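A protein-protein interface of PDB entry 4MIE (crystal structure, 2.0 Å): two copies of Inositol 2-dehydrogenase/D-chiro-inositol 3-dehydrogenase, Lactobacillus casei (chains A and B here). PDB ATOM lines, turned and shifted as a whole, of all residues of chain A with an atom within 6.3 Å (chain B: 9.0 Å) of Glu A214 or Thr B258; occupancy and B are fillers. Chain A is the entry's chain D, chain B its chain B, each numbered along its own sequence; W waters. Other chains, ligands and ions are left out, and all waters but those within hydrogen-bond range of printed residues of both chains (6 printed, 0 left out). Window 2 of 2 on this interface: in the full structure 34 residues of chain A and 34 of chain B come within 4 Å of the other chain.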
ATOM      1  N   ASN A 171      11.719 -10.301   5.015  1.00  0.00           N
ATOM      2  CA  ASN A 171      10.364 -10.193   4.505  1.00  0.00           C
ATOM      3  C   ASN A 171      10.395 -10.058   2.993  1.00  0.00           C
ATOM      4  O   ASN A 171      11.375  -9.598   2.437  1.00  0.00           O
ATOM      5  CB  ASN A 171       9.639  -8.972   5.096  1.00  0.00           C
ATOM      6  CG  ASN A 171       8.904  -9.266   6.410  1.00  0.00           C
ATOM      7  OD1 ASN A 171       8.096 -10.188   6.506  1.00  0.00           O
ATOM      8  ND2 ASN A 171       9.173  -8.454   7.419  1.00  0.00           N
ATOM      9  N   GLN A 211       4.364 -24.182   8.490  1.00  0.00           N
ATOM     10  CA  GLN A 211       4.202 -22.900   7.824  1.00  0.00           C
ATOM     11  C   GLN A 211       4.261 -21.736   8.805  1.00  0.00           C
ATOM     12  O   GLN A 211       3.651 -21.783   9.831  1.00  0.00           O
ATOM     13  CB  GLN A 211       2.884 -22.893   7.062  1.00  0.00           C
ATOM     14  CG  GLN A 211       2.491 -21.577   6.473  1.00  0.00           C
ATOM     15  CD  GLN A 211       3.198 -21.268   5.172  1.00  0.00           C
ATOM     16  OE1 GLN A 211       4.156 -21.909   4.799  1.00  0.00           O
ATOM     17  NE2 GLN A 211       2.702 -20.274   4.477  1.00  0.00           N
ATOM     18  N   SER A 212       5.014 -20.700   8.475  1.00  0.00           N
ATOM     19  CA  SER A 212       5.109 -19.529   9.329  1.00  0.00           C
ATOM     20  C   SER A 212       3.874 -18.666   9.301  1.00  0.00           C
ATOM     21  O   SER A 212       3.305 -18.423   8.266  1.00  0.00           O
ATOM     22  CB  SER A 212       6.295 -18.655   8.952  1.00  0.00           C
ATOM     23  OG  SER A 212       6.349 -17.492   9.729  1.00  0.00           O
ATOM     24  N   ALA A 213       3.511 -18.156  10.460  1.00  0.00           N
ATOM     25  CA  ALA A 213       2.443 -17.184  10.569  1.00  0.00           C
ATOM     26  C   ALA A 213       2.783 -15.832   9.924  1.00  0.00           C
ATOM     27  O   ALA A 213       1.904 -15.068   9.621  1.00  0.00           O
ATOM     28  CB  ALA A 213       2.042 -17.004  12.015  1.00  0.00           C
ATOM     29  N   GLU A 214       4.065 -15.564   9.713  1.00  0.00           N
ATOM     30  CA  GLU A 214       4.527 -14.313   9.105  1.00  0.00           C
ATOM     31  C   GLU A 214       4.313 -14.218   7.582  1.00  0.00           C
ATOM     32  O   GLU A 214       4.495 -13.179   7.005  1.00  0.00           O
ATOM     33  CB  GLU A 214       5.981 -14.042   9.437  1.00  0.00           C
ATOM     34  CG  GLU A 214       6.304 -14.024  10.910  1.00  0.00           C
ATOM     35  CD  GLU A 214       5.504 -13.006  11.704  1.00  0.00           C
ATOM     36  OE1 GLU A 214       5.158 -11.964  11.162  1.00  0.00           O
ATOM     37  OE2 GLU A 214       5.244 -13.250  12.873  1.00  0.00           O
ATOM     38  N   VAL A 215       3.911 -15.313   6.957  1.00  0.00           N
ATOM     39  CA  VAL A 215       3.644 -15.307   5.530  1.00  0.00           C
ATOM     40  C   VAL A 215       2.421 -14.453   5.210  1.00  0.00           C
ATOM     41  O   VAL A 215       1.380 -14.593   5.814  1.00  0.00           O
ATOM     42  CB  VAL A 215       3.499 -16.721   4.957  1.00  0.00           C
ATOM     43  CG1 VAL A 215       3.104 -16.684   3.484  1.00  0.00           C
ATOM     44  CG2 VAL A 215       4.750 -17.475   5.111  1.00  0.00           C
ATOM     45  N   ARG A 216       2.580 -13.573   4.237  1.00  0.00           N
ATOM     46  CA  ARG A 216       1.504 -12.724   3.789  1.00  0.00           C
ATOM     47  C   ARG A 216       1.167 -12.899   2.322  1.00  0.00           C
ATOM     48  O   ARG A 216       0.354 -12.168   1.800  1.00  0.00           O
ATOM     49  CB  ARG A 216       1.866 -11.275   4.024  1.00  0.00           C
ATOM     50  CG  ARG A 216       2.350 -10.968   5.398  1.00  0.00           C
ATOM     51  CD  ARG A 216       2.577  -9.484   5.582  1.00  0.00           C
ATOM     52  NE  ARG A 216       2.678  -8.815   4.300  1.00  0.00           N
ATOM     53  CZ  ARG A 216       1.884  -7.843   3.898  1.00  0.00           C
ATOM     54  NH1 ARG A 216       0.945  -7.393   4.693  1.00  0.00           N
ATOM     55  NH2 ARG A 216       2.046  -7.316   2.699  1.00  0.00           N
ATOM     56  N   ASN A 217       1.808 -13.853   1.664  1.00  0.00           N
ATOM     57  CA  ASN A 217       1.632 -14.054   0.243  1.00  0.00           C
ATOM     58  C   ASN A 217       0.955 -15.369  -0.032  1.00  0.00           C
ATOM     59  O   ASN A 217       1.460 -16.412   0.344  1.00  0.00           O
ATOM     60  CB  ASN A 217       2.967 -14.074  -0.479  1.00  0.00           C
ATOM     61  CG  ASN A 217       3.675 -12.756  -0.455  1.00  0.00           C
ATOM     62  OD1 ASN A 217       3.508 -11.966   0.451  1.00  0.00           O
ATOM     63  ND2 ASN A 217       4.498 -12.526  -1.460  1.00  0.00           N
ATOM     64  N   HIS A 241      14.447 -19.324   4.233  1.00  0.00           N
ATOM     65  CA  HIS A 241      13.550 -18.640   5.148  1.00  0.00           C
ATOM     66  C   HIS A 241      13.468 -17.158   4.815  1.00  0.00           C
ATOM     67  O   HIS A 241      14.347 -16.396   5.153  1.00  0.00           O
ATOM     68  CB  HIS A 241      14.007 -18.842   6.584  1.00  0.00           C
ATOM     69  CG  HIS A 241      12.974 -18.504   7.607  1.00  0.00           C
ATOM     70  ND1 HIS A 241      13.246 -18.473   8.950  1.00  0.00           N
ATOM     71  CD2 HIS A 241      11.670 -18.184   7.482  1.00  0.00           C
ATOM     72  CE1 HIS A 241      12.156 -18.151   9.608  1.00  0.00           C
ATOM     73  NE2 HIS A 241      11.183 -17.974   8.741  1.00  0.00           N
ATOM     74  N   THR A 243      10.669 -14.954   5.376  1.00  0.00           N
ATOM     75  CA  THR A 243       9.885 -14.113   6.261  1.00  0.00           C
ATOM     76  C   THR A 243      10.423 -14.173   7.677  1.00  0.00           C
ATOM     77  O   THR A 243       9.677 -14.071   8.610  1.00  0.00           O
ATOM     78  CB  THR A 243       8.395 -14.508   6.263  1.00  0.00           C
ATOM     79  OG1 THR A 243       8.219 -15.796   6.828  1.00  0.00           O
ATOM     80  CG2 THR A 243       7.857 -14.491   4.862  1.00  0.00           C
ATOM     81  N   ALA A 244      11.731 -14.323   7.804  1.00  0.00           N
ATOM     82  CA  ALA A 244      12.383 -14.568   9.085  1.00  0.00           C
ATOM     83  C   ALA A 244      12.374 -13.396  10.060  1.00  0.00           C
ATOM     84  O   ALA A 244      12.607 -13.578  11.229  1.00  0.00           O
ATOM     85  CB  ALA A 244      13.792 -15.071   8.874  1.00  0.00           C
ATOM     86  N   GLN A 245      12.103 -12.210   9.533  1.00  0.00           N
ATOM     87  CA  GLN A 245      11.944 -10.974  10.291  1.00  0.00           C
ATOM     88  C   GLN A 245      13.227 -10.313  10.825  1.00  0.00           C
ATOM     89  O   GLN A 245      13.406  -9.124  10.705  1.00  0.00           O
ATOM     90  CB  GLN A 245      10.926 -11.135  11.432  1.00  0.00           C
ATOM     91  CG  GLN A 245       9.577 -11.643  11.033  1.00  0.00           C
ATOM     92  CD  GLN A 245       8.914 -10.801   9.976  1.00  0.00           C
ATOM     93  OE1 GLN A 245       8.825  -9.609  10.105  1.00  0.00           O
ATOM     94  NE2 GLN A 245       8.454 -11.430   8.925  1.00  0.00           N
ATOM     95  N   TYR A 246      14.104 -11.097  11.417  1.00  0.00           N
ATOM     96  CA  TYR A 246      15.222 -10.554  12.152  1.00  0.00           C
ATOM     97  C   TYR A 246      16.306  -9.867  11.306  1.00  0.00           C
ATOM     98  O   TYR A 246      16.954  -8.960  11.762  1.00  0.00           O
ATOM     99  CB  TYR A 246      15.841 -11.621  13.057  1.00  0.00           C
ATOM    100  CG  TYR A 246      16.815 -12.564  12.389  1.00  0.00           C
ATOM    101  CD1 TYR A 246      18.142 -12.220  12.222  1.00  0.00           C
ATOM    102  CD2 TYR A 246      16.416 -13.807  11.956  1.00  0.00           C
ATOM    103  CE1 TYR A 246      19.027 -13.084  11.626  1.00  0.00           C
ATOM    104  CE2 TYR A 246      17.285 -14.664  11.363  1.00  0.00           C
ATOM    105  CZ  TYR A 246      18.591 -14.311  11.197  1.00  0.00           C
ATOM    106  OH  TYR A 246      19.473 -15.161  10.601  1.00  0.00           O
ATOM    107  N   LEU B 152      13.165 -19.834  24.268  1.00  0.00           N
ATOM    108  CA  LEU B 152      12.194 -20.206  23.274  1.00  0.00           C
ATOM    109  C   LEU B 152      10.785 -20.094  23.830  1.00  0.00           C
ATOM    110  O   LEU B 152       9.907 -19.537  23.212  1.00  0.00           O
ATOM    111  CB  LEU B 152      12.458 -21.627  22.828  1.00  0.00           C
ATOM    112  CG  LEU B 152      11.407 -22.216  21.913  1.00  0.00           C
ATOM    113  CD1 LEU B 152      11.278 -21.415  20.652  1.00  0.00           C
ATOM    114  CD2 LEU B 152      11.694 -23.670  21.649  1.00  0.00           C
ATOM    115  N   GLY B 155       8.395 -17.100  23.835  1.00  0.00           N
ATOM    116  CA  GLY B 155       7.710 -16.697  22.631  1.00  0.00           C
ATOM    117  C   GLY B 155       8.443 -15.655  21.814  1.00  0.00           C
ATOM    118  O   GLY B 155       7.973 -15.220  20.797  1.00  0.00           O
ATOM    119  N   ILE B 156       9.625 -15.291  22.249  1.00  0.00           N
ATOM    120  CA  ILE B 156      10.344 -14.216  21.623  1.00  0.00           C
ATOM    121  C   ILE B 156      10.730 -14.442  20.144  1.00  0.00           C
ATOM    122  O   ILE B 156      10.893 -13.501  19.415  1.00  0.00           O
ATOM    123  CB  ILE B 156      11.550 -13.793  22.465  1.00  0.00           C
ATOM    124  CG1 ILE B 156      11.996 -12.388  22.058  1.00  0.00           C
ATOM    125  CG2 ILE B 156      12.651 -14.846  22.412  1.00  0.00           C
ATOM    126  CD1 ILE B 156      13.150 -11.908  22.760  1.00  0.00           C
ATOM    127  N   ILE B 157      10.837 -15.680  19.703  1.00  0.00           N
ATOM    128  CA  ILE B 157      11.062 -15.930  18.287  1.00  0.00           C
ATOM    129  C   ILE B 157       9.875 -16.531  17.559  1.00  0.00           C
ATOM    130  O   ILE B 157       9.990 -16.986  16.443  1.00  0.00           O
ATOM    131  CB  ILE B 157      12.344 -16.766  18.019  1.00  0.00           C
ATOM    132  CG1 ILE B 157      12.229 -18.179  18.608  1.00  0.00           C
ATOM    133  CG2 ILE B 157      13.543 -16.022  18.530  1.00  0.00           C
ATOM    134  CD1 ILE B 157      13.196 -19.144  18.076  1.00  0.00           C
ATOM    135  N   GLY B 158       8.722 -16.485  18.192  1.00  0.00           N
ATOM    136  CA  GLY B 158       7.554 -17.121  17.650  1.00  0.00           C
ATOM    137  C   GLY B 158       7.638 -18.631  17.735  1.00  0.00           C
ATOM    138  O   GLY B 158       8.388 -19.179  18.507  1.00  0.00           O
ATOM    139  N   ALA B 159       6.834 -19.291  16.931  1.00  0.00           N
ATOM    140  CA  ALA B 159       6.775 -20.730  16.950  1.00  0.00           C
ATOM    141  C   ALA B 159       8.009 -21.348  16.291  1.00  0.00           C
ATOM    142  O   ALA B 159       8.515 -20.820  15.326  1.00  0.00           O
ATOM    143  CB  ALA B 159       5.529 -21.201  16.281  1.00  0.00           C
ATOM    144  N   PRO B 160       8.491 -22.468  16.840  1.00  0.00           N
ATOM    145  CA  PRO B 160       9.651 -23.129  16.258  1.00  0.00           C
ATOM    146  C   PRO B 160       9.240 -23.894  14.990  1.00  0.00           C
ATOM    147  O   PRO B 160       8.357 -24.727  15.038  1.00  0.00           O
ATOM    148  CB  PRO B 160      10.117 -24.050  17.378  1.00  0.00           C
ATOM    149  CG  PRO B 160       8.865 -24.362  18.145  1.00  0.00           C
ATOM    150  CD  PRO B 160       7.990 -23.171  18.029  1.00  0.00           C
ATOM    151  N   LEU B 161       9.883 -23.571  13.880  1.00  0.00           N
ATOM    152  CA  LEU B 161       9.539 -24.109  12.575  1.00  0.00           C
ATOM    153  C   LEU B 161      10.505 -25.198  12.122  1.00  0.00           C
ATOM    154  O   LEU B 161      10.108 -26.176  11.533  1.00  0.00           O
ATOM    155  CB  LEU B 161       9.511 -22.991  11.538  1.00  0.00           C
ATOM    156  CG  LEU B 161       8.648 -21.775  11.852  1.00  0.00           C
ATOM    157  CD1 LEU B 161       8.712 -20.757  10.754  1.00  0.00           C
ATOM    158  CD2 LEU B 161       7.253 -22.200  12.092  1.00  0.00           C
ATOM    159  N   VAL B 254      17.501 -23.298  16.826  1.00  0.00           N
ATOM    160  CA  VAL B 254      16.067 -23.280  16.621  1.00  0.00           C
ATOM    161  C   VAL B 254      15.657 -22.118  15.720  1.00  0.00           C
ATOM    162  O   VAL B 254      15.991 -20.978  15.970  1.00  0.00           O
ATOM    163  CB  VAL B 254      15.280 -23.265  17.940  1.00  0.00           C
ATOM    164  CG1 VAL B 254      13.822 -23.242  17.681  1.00  0.00           C
ATOM    165  CG2 VAL B 254      15.639 -24.457  18.784  1.00  0.00           C
ATOM    166  N   ILE B 255      14.952 -22.463  14.659  1.00  0.00           N
ATOM    167  CA  ILE B 255      14.484 -21.522  13.668  1.00  0.00           C
ATOM    168  C   ILE B 255      13.031 -21.185  13.939  1.00  0.00           C
ATOM    169  O   ILE B 255      12.166 -22.026  13.810  1.00  0.00           O
ATOM    170  CB  ILE B 255      14.582 -22.073  12.225  1.00  0.00           C
ATOM    171  CG1 ILE B 255      15.966 -22.639  11.899  1.00  0.00           C
ATOM    172  CG2 ILE B 255      14.140 -21.028  11.244  1.00  0.00           C
ATOM    173  CD1 ILE B 255      17.093 -21.688  12.101  1.00  0.00           C
ATOM    174  N   GLY B 256      12.793 -19.941  14.306  1.00  0.00           N
ATOM    175  CA  GLY B 256      11.469 -19.469  14.644  1.00  0.00           C
ATOM    176  C   GLY B 256      10.871 -18.507  13.646  1.00  0.00           C
ATOM    177  O   GLY B 256      11.548 -18.027  12.763  1.00  0.00           O
ATOM    178  N   GLU B 257       9.585 -18.238  13.800  1.00  0.00           N
ATOM    179  CA  GLU B 257       8.862 -17.343  12.905  1.00  0.00           C
ATOM    180  C   GLU B 257       9.480 -15.939  12.805  1.00  0.00           C
ATOM    181  O   GLU B 257       9.523 -15.358  11.747  1.00  0.00           O
ATOM    182  CB  GLU B 257       7.392 -17.247  13.313  1.00  0.00           C
ATOM    183  CG  GLU B 257       6.612 -18.523  13.163  1.00  0.00           C
ATOM    184  CD  GLU B 257       5.252 -18.482  13.811  1.00  0.00           C
ATOM    185  OE1 GLU B 257       5.155 -18.038  14.960  1.00  0.00           O
ATOM    186  OE2 GLU B 257       4.303 -18.911  13.172  1.00  0.00           O
ATOM    187  N   THR B 258       9.956 -15.425  13.928  1.00  0.00           N
ATOM    188  CA  THR B 258      10.425 -14.053  14.013  1.00  0.00           C
ATOM    189  C   THR B 258      11.871 -13.919  14.472  1.00  0.00           C
ATOM    190  O   THR B 258      12.361 -12.826  14.665  1.00  0.00           O
ATOM    191  CB  THR B 258       9.581 -13.235  14.985  1.00  0.00           C
ATOM    192  OG1 THR B 258       9.754 -13.756  16.295  1.00  0.00           O
ATOM    193  CG2 THR B 258       8.148 -13.257  14.602  1.00  0.00           C
ATOM    194  N   GLY B 259      12.533 -15.053  14.641  1.00  0.00           N
ATOM    195  CA  GLY B 259      13.911 -15.067  15.051  1.00  0.00           C
ATOM    196  C   GLY B 259      14.552 -16.439  15.141  1.00  0.00           C
ATOM    197  O   GLY B 259      13.928 -17.437  14.835  1.00  0.00           O
ATOM    198  N   GLU B 260      15.814 -16.464  15.536  1.00  0.00           N
ATOM    199  CA  GLU B 260      16.509 -17.708  15.808  1.00  0.00           C
ATOM    200  C   GLU B 260      17.169 -17.729  17.191  1.00  0.00           C
ATOM    201  O   GLU B 260      17.492 -16.695  17.737  1.00  0.00           O
ATOM    202  CB  GLU B 260      17.570 -17.991  14.746  1.00  0.00           C
ATOM    203  CG  GLU B 260      17.083 -18.083  13.328  1.00  0.00           C
ATOM    204  CD  GLU B 260      18.210 -18.337  12.326  1.00  0.00           C
ATOM    205  OE1 GLU B 260      19.362 -18.471  12.726  1.00  0.00           O
ATOM    206  OE2 GLU B 260      17.924 -18.388  11.132  1.00  0.00           O
ATOM    207  N   LEU B 261      17.380 -18.936  17.710  1.00  0.00           N
ATOM    208  CA  LEU B 261      18.178 -19.179  18.908  1.00  0.00           C
ATOM    209  C   LEU B 261      19.218 -20.257  18.644  1.00  0.00           C
ATOM    210  O   LEU B 261      18.949 -21.209  17.941  1.00  0.00           O
ATOM    211  CB  LEU B 261      17.300 -19.638  20.054  1.00  0.00           C
ATOM    212  CG  LEU B 261      16.360 -18.624  20.686  1.00  0.00           C
ATOM    213  CD1 LEU B 261      15.201 -19.298  21.364  1.00  0.00           C
ATOM    214  CD2 LEU B 261      17.119 -17.761  21.641  1.00  0.00           C
HETATM  215  O   HOH W   1      15.606 -17.662  10.511  1.00  0.00           O
HETATM  216  O   HOH W   2       4.897 -15.148  14.710  1.00  0.00           O
HETATM  217  O   HOH W   3      12.798 -10.171  14.272  1.00  0.00           O
HETATM  218  O   HOH W   4      13.655 -16.198  11.989  1.00  0.00           O
HETATM  219  O   HOH W   5       3.001 -21.221  12.505  1.00  0.00           O
HETATM  220  O   HOH W   6       8.735 -16.610   9.476  1.00  0.00           O
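O of Glu B257 sits close to O of Thr A243.
The side-chain carboxylate (OE2) of Glu B257 sits at hydrogen-bond distance from the backbone NH (N) of Ala A213, 2.9 Å away.
The backbone carbonyl oxygen of Ile B157 sits at hydrogen-bond distance from the backbone NH of Thr B258, at 3.0 Å.
The backbone carbonyl oxygen (O) of Thr A243 lies within hydrogen-bond range of the side-chain amide nitrogen (NE2) of Gln A245.
The backbone NH (N) of Gly B158 lies within hydrogen-bond range of the side-chain hydroxyl (OG1) of Thr B258, at 3.5 Å.
NE2 of Gln A245 lies within hydrogen-bond range of OD1 of Asn A171 (2.7 Å).
O of Ile B156 is in hydrogen-bond range of OG1 of Thr B258, 3.3 Å away.
OG of Ser A212 sits at hydrogen-bond distance from N of Glu A214 (3.0 Å).
CD1 of Leu B161 touches CB of Ser A212, at 3.7 Å.
CG of Glu B257 touches OG of Ser A212 (3.6 Å).
Glu A214 touches Glu B257.
Thr B258 touches Glu A214 (CG2 to OE2, 3.4 Å).
His A241 touches Ile B255.
Ala A244 touches Glu B257.
O of Ala A244 touches C of Thr B258 (3.3 Å).
Ala A244 touches Gly B259 (O to N, 3.7 Å).
Gln A245 touches Glu B257 (CG to O, 3.8 Å).
Thr B258 touches Gln A245 (O to CB, 3.9 Å).
Of chain B, only Glu B257 (2.9 Å) comes within 4 Å of Ala A213.
Of chain B, only Glu B257 and Thr B258 come within 4 Å of Glu A214.
No residue of chain B comes within 4 Å of Val A215.
Of the printed residues of chain B, Ala A244 touches Glu B257 (3.6 Å), Thr B258 (3.3 Å) and Gly B259 (3.7 Å).
Printed residues of chain B within 4 Å of Gln A245: Glu B257 and Thr B258.
Printed residues of chain B within 4 Å of Tyr A246: Glu B260 (3.6 Å).
Of the printed residues of chain A, Ile B255 touches His A241 (3.5 Å).
Of the printed residues of chain A, Thr B258 touches Glu A214 (3.4 Å), Ala A244 (3.3 Å) and Gln A245 (3.9 Å).
Of the printed residues of chain A, Glu B260 touches Tyr A246 (3.6 Å).
The nearest printed residue of chain B that does not touch Ser A212 is Thr B258 (5.9 Å).
Of the 13 printed residues of chain A, 8 touch a printed residue of chain B.
Hydrophobic or aromatic side chains of chain A within 4 Å of the printed part of chain B: Ala A213, His A241 and Tyr A246.
Printed residues of chain B that touch a printed residue of chain A: Leu B161, Ile B255, Gly B256, Glu B257, Thr B258, Gly B259 and Glu B260.
Hydrophobic or aromatic side chains of chain B that line the printed part of chain A: Leu B161 and Ile B255.
Among the printed residues, no Asp or Glu carboxylate lies within 4 Å of a Lys or Arg side-chain nitrogen of the other chain.
No position is printed for both chains.
Of the 14 pairs that touch across the chains among the printed residues, none has its exchanged pair printed and touching as well.
Water W1 lies within hydrogen-bond range of the side-chain carboxylate of Glu B260 (2.5 Å) and a ring nitrogen (ND1) of His A241 (2.9 Å).
Water W6 lies within hydrogen-bond range of OG of Ser A212 (2.6 Å), O of Glu B257 (2.7 Å), OG1 of Thr A243 (2.8 Å) and NE2 of His A241 (2.9 Å).
Water W2 bridges OE2 of Glu A214 and OE1 of Glu B257.
Water W3 lies within hydrogen-bond range of O of Thr B258 (2.7 Å) and N of Tyr A246 (3.3 Å).
Water W5 bridges the side-chain carboxylate (OE2) of Glu B257 (2.7 Å) and the backbone carbonyl oxygen (O) of Gln A211 (2.8 Å).
Water W4 lies within hydrogen-bond range of the backbone carbonyl oxygen (O) of Gly B256 (2.9 Å), the backbone carbonyl oxygen (O) of Ala A244 (2.9 Å) and the backbone NH (N) of Gly B259 (3.1 Å).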
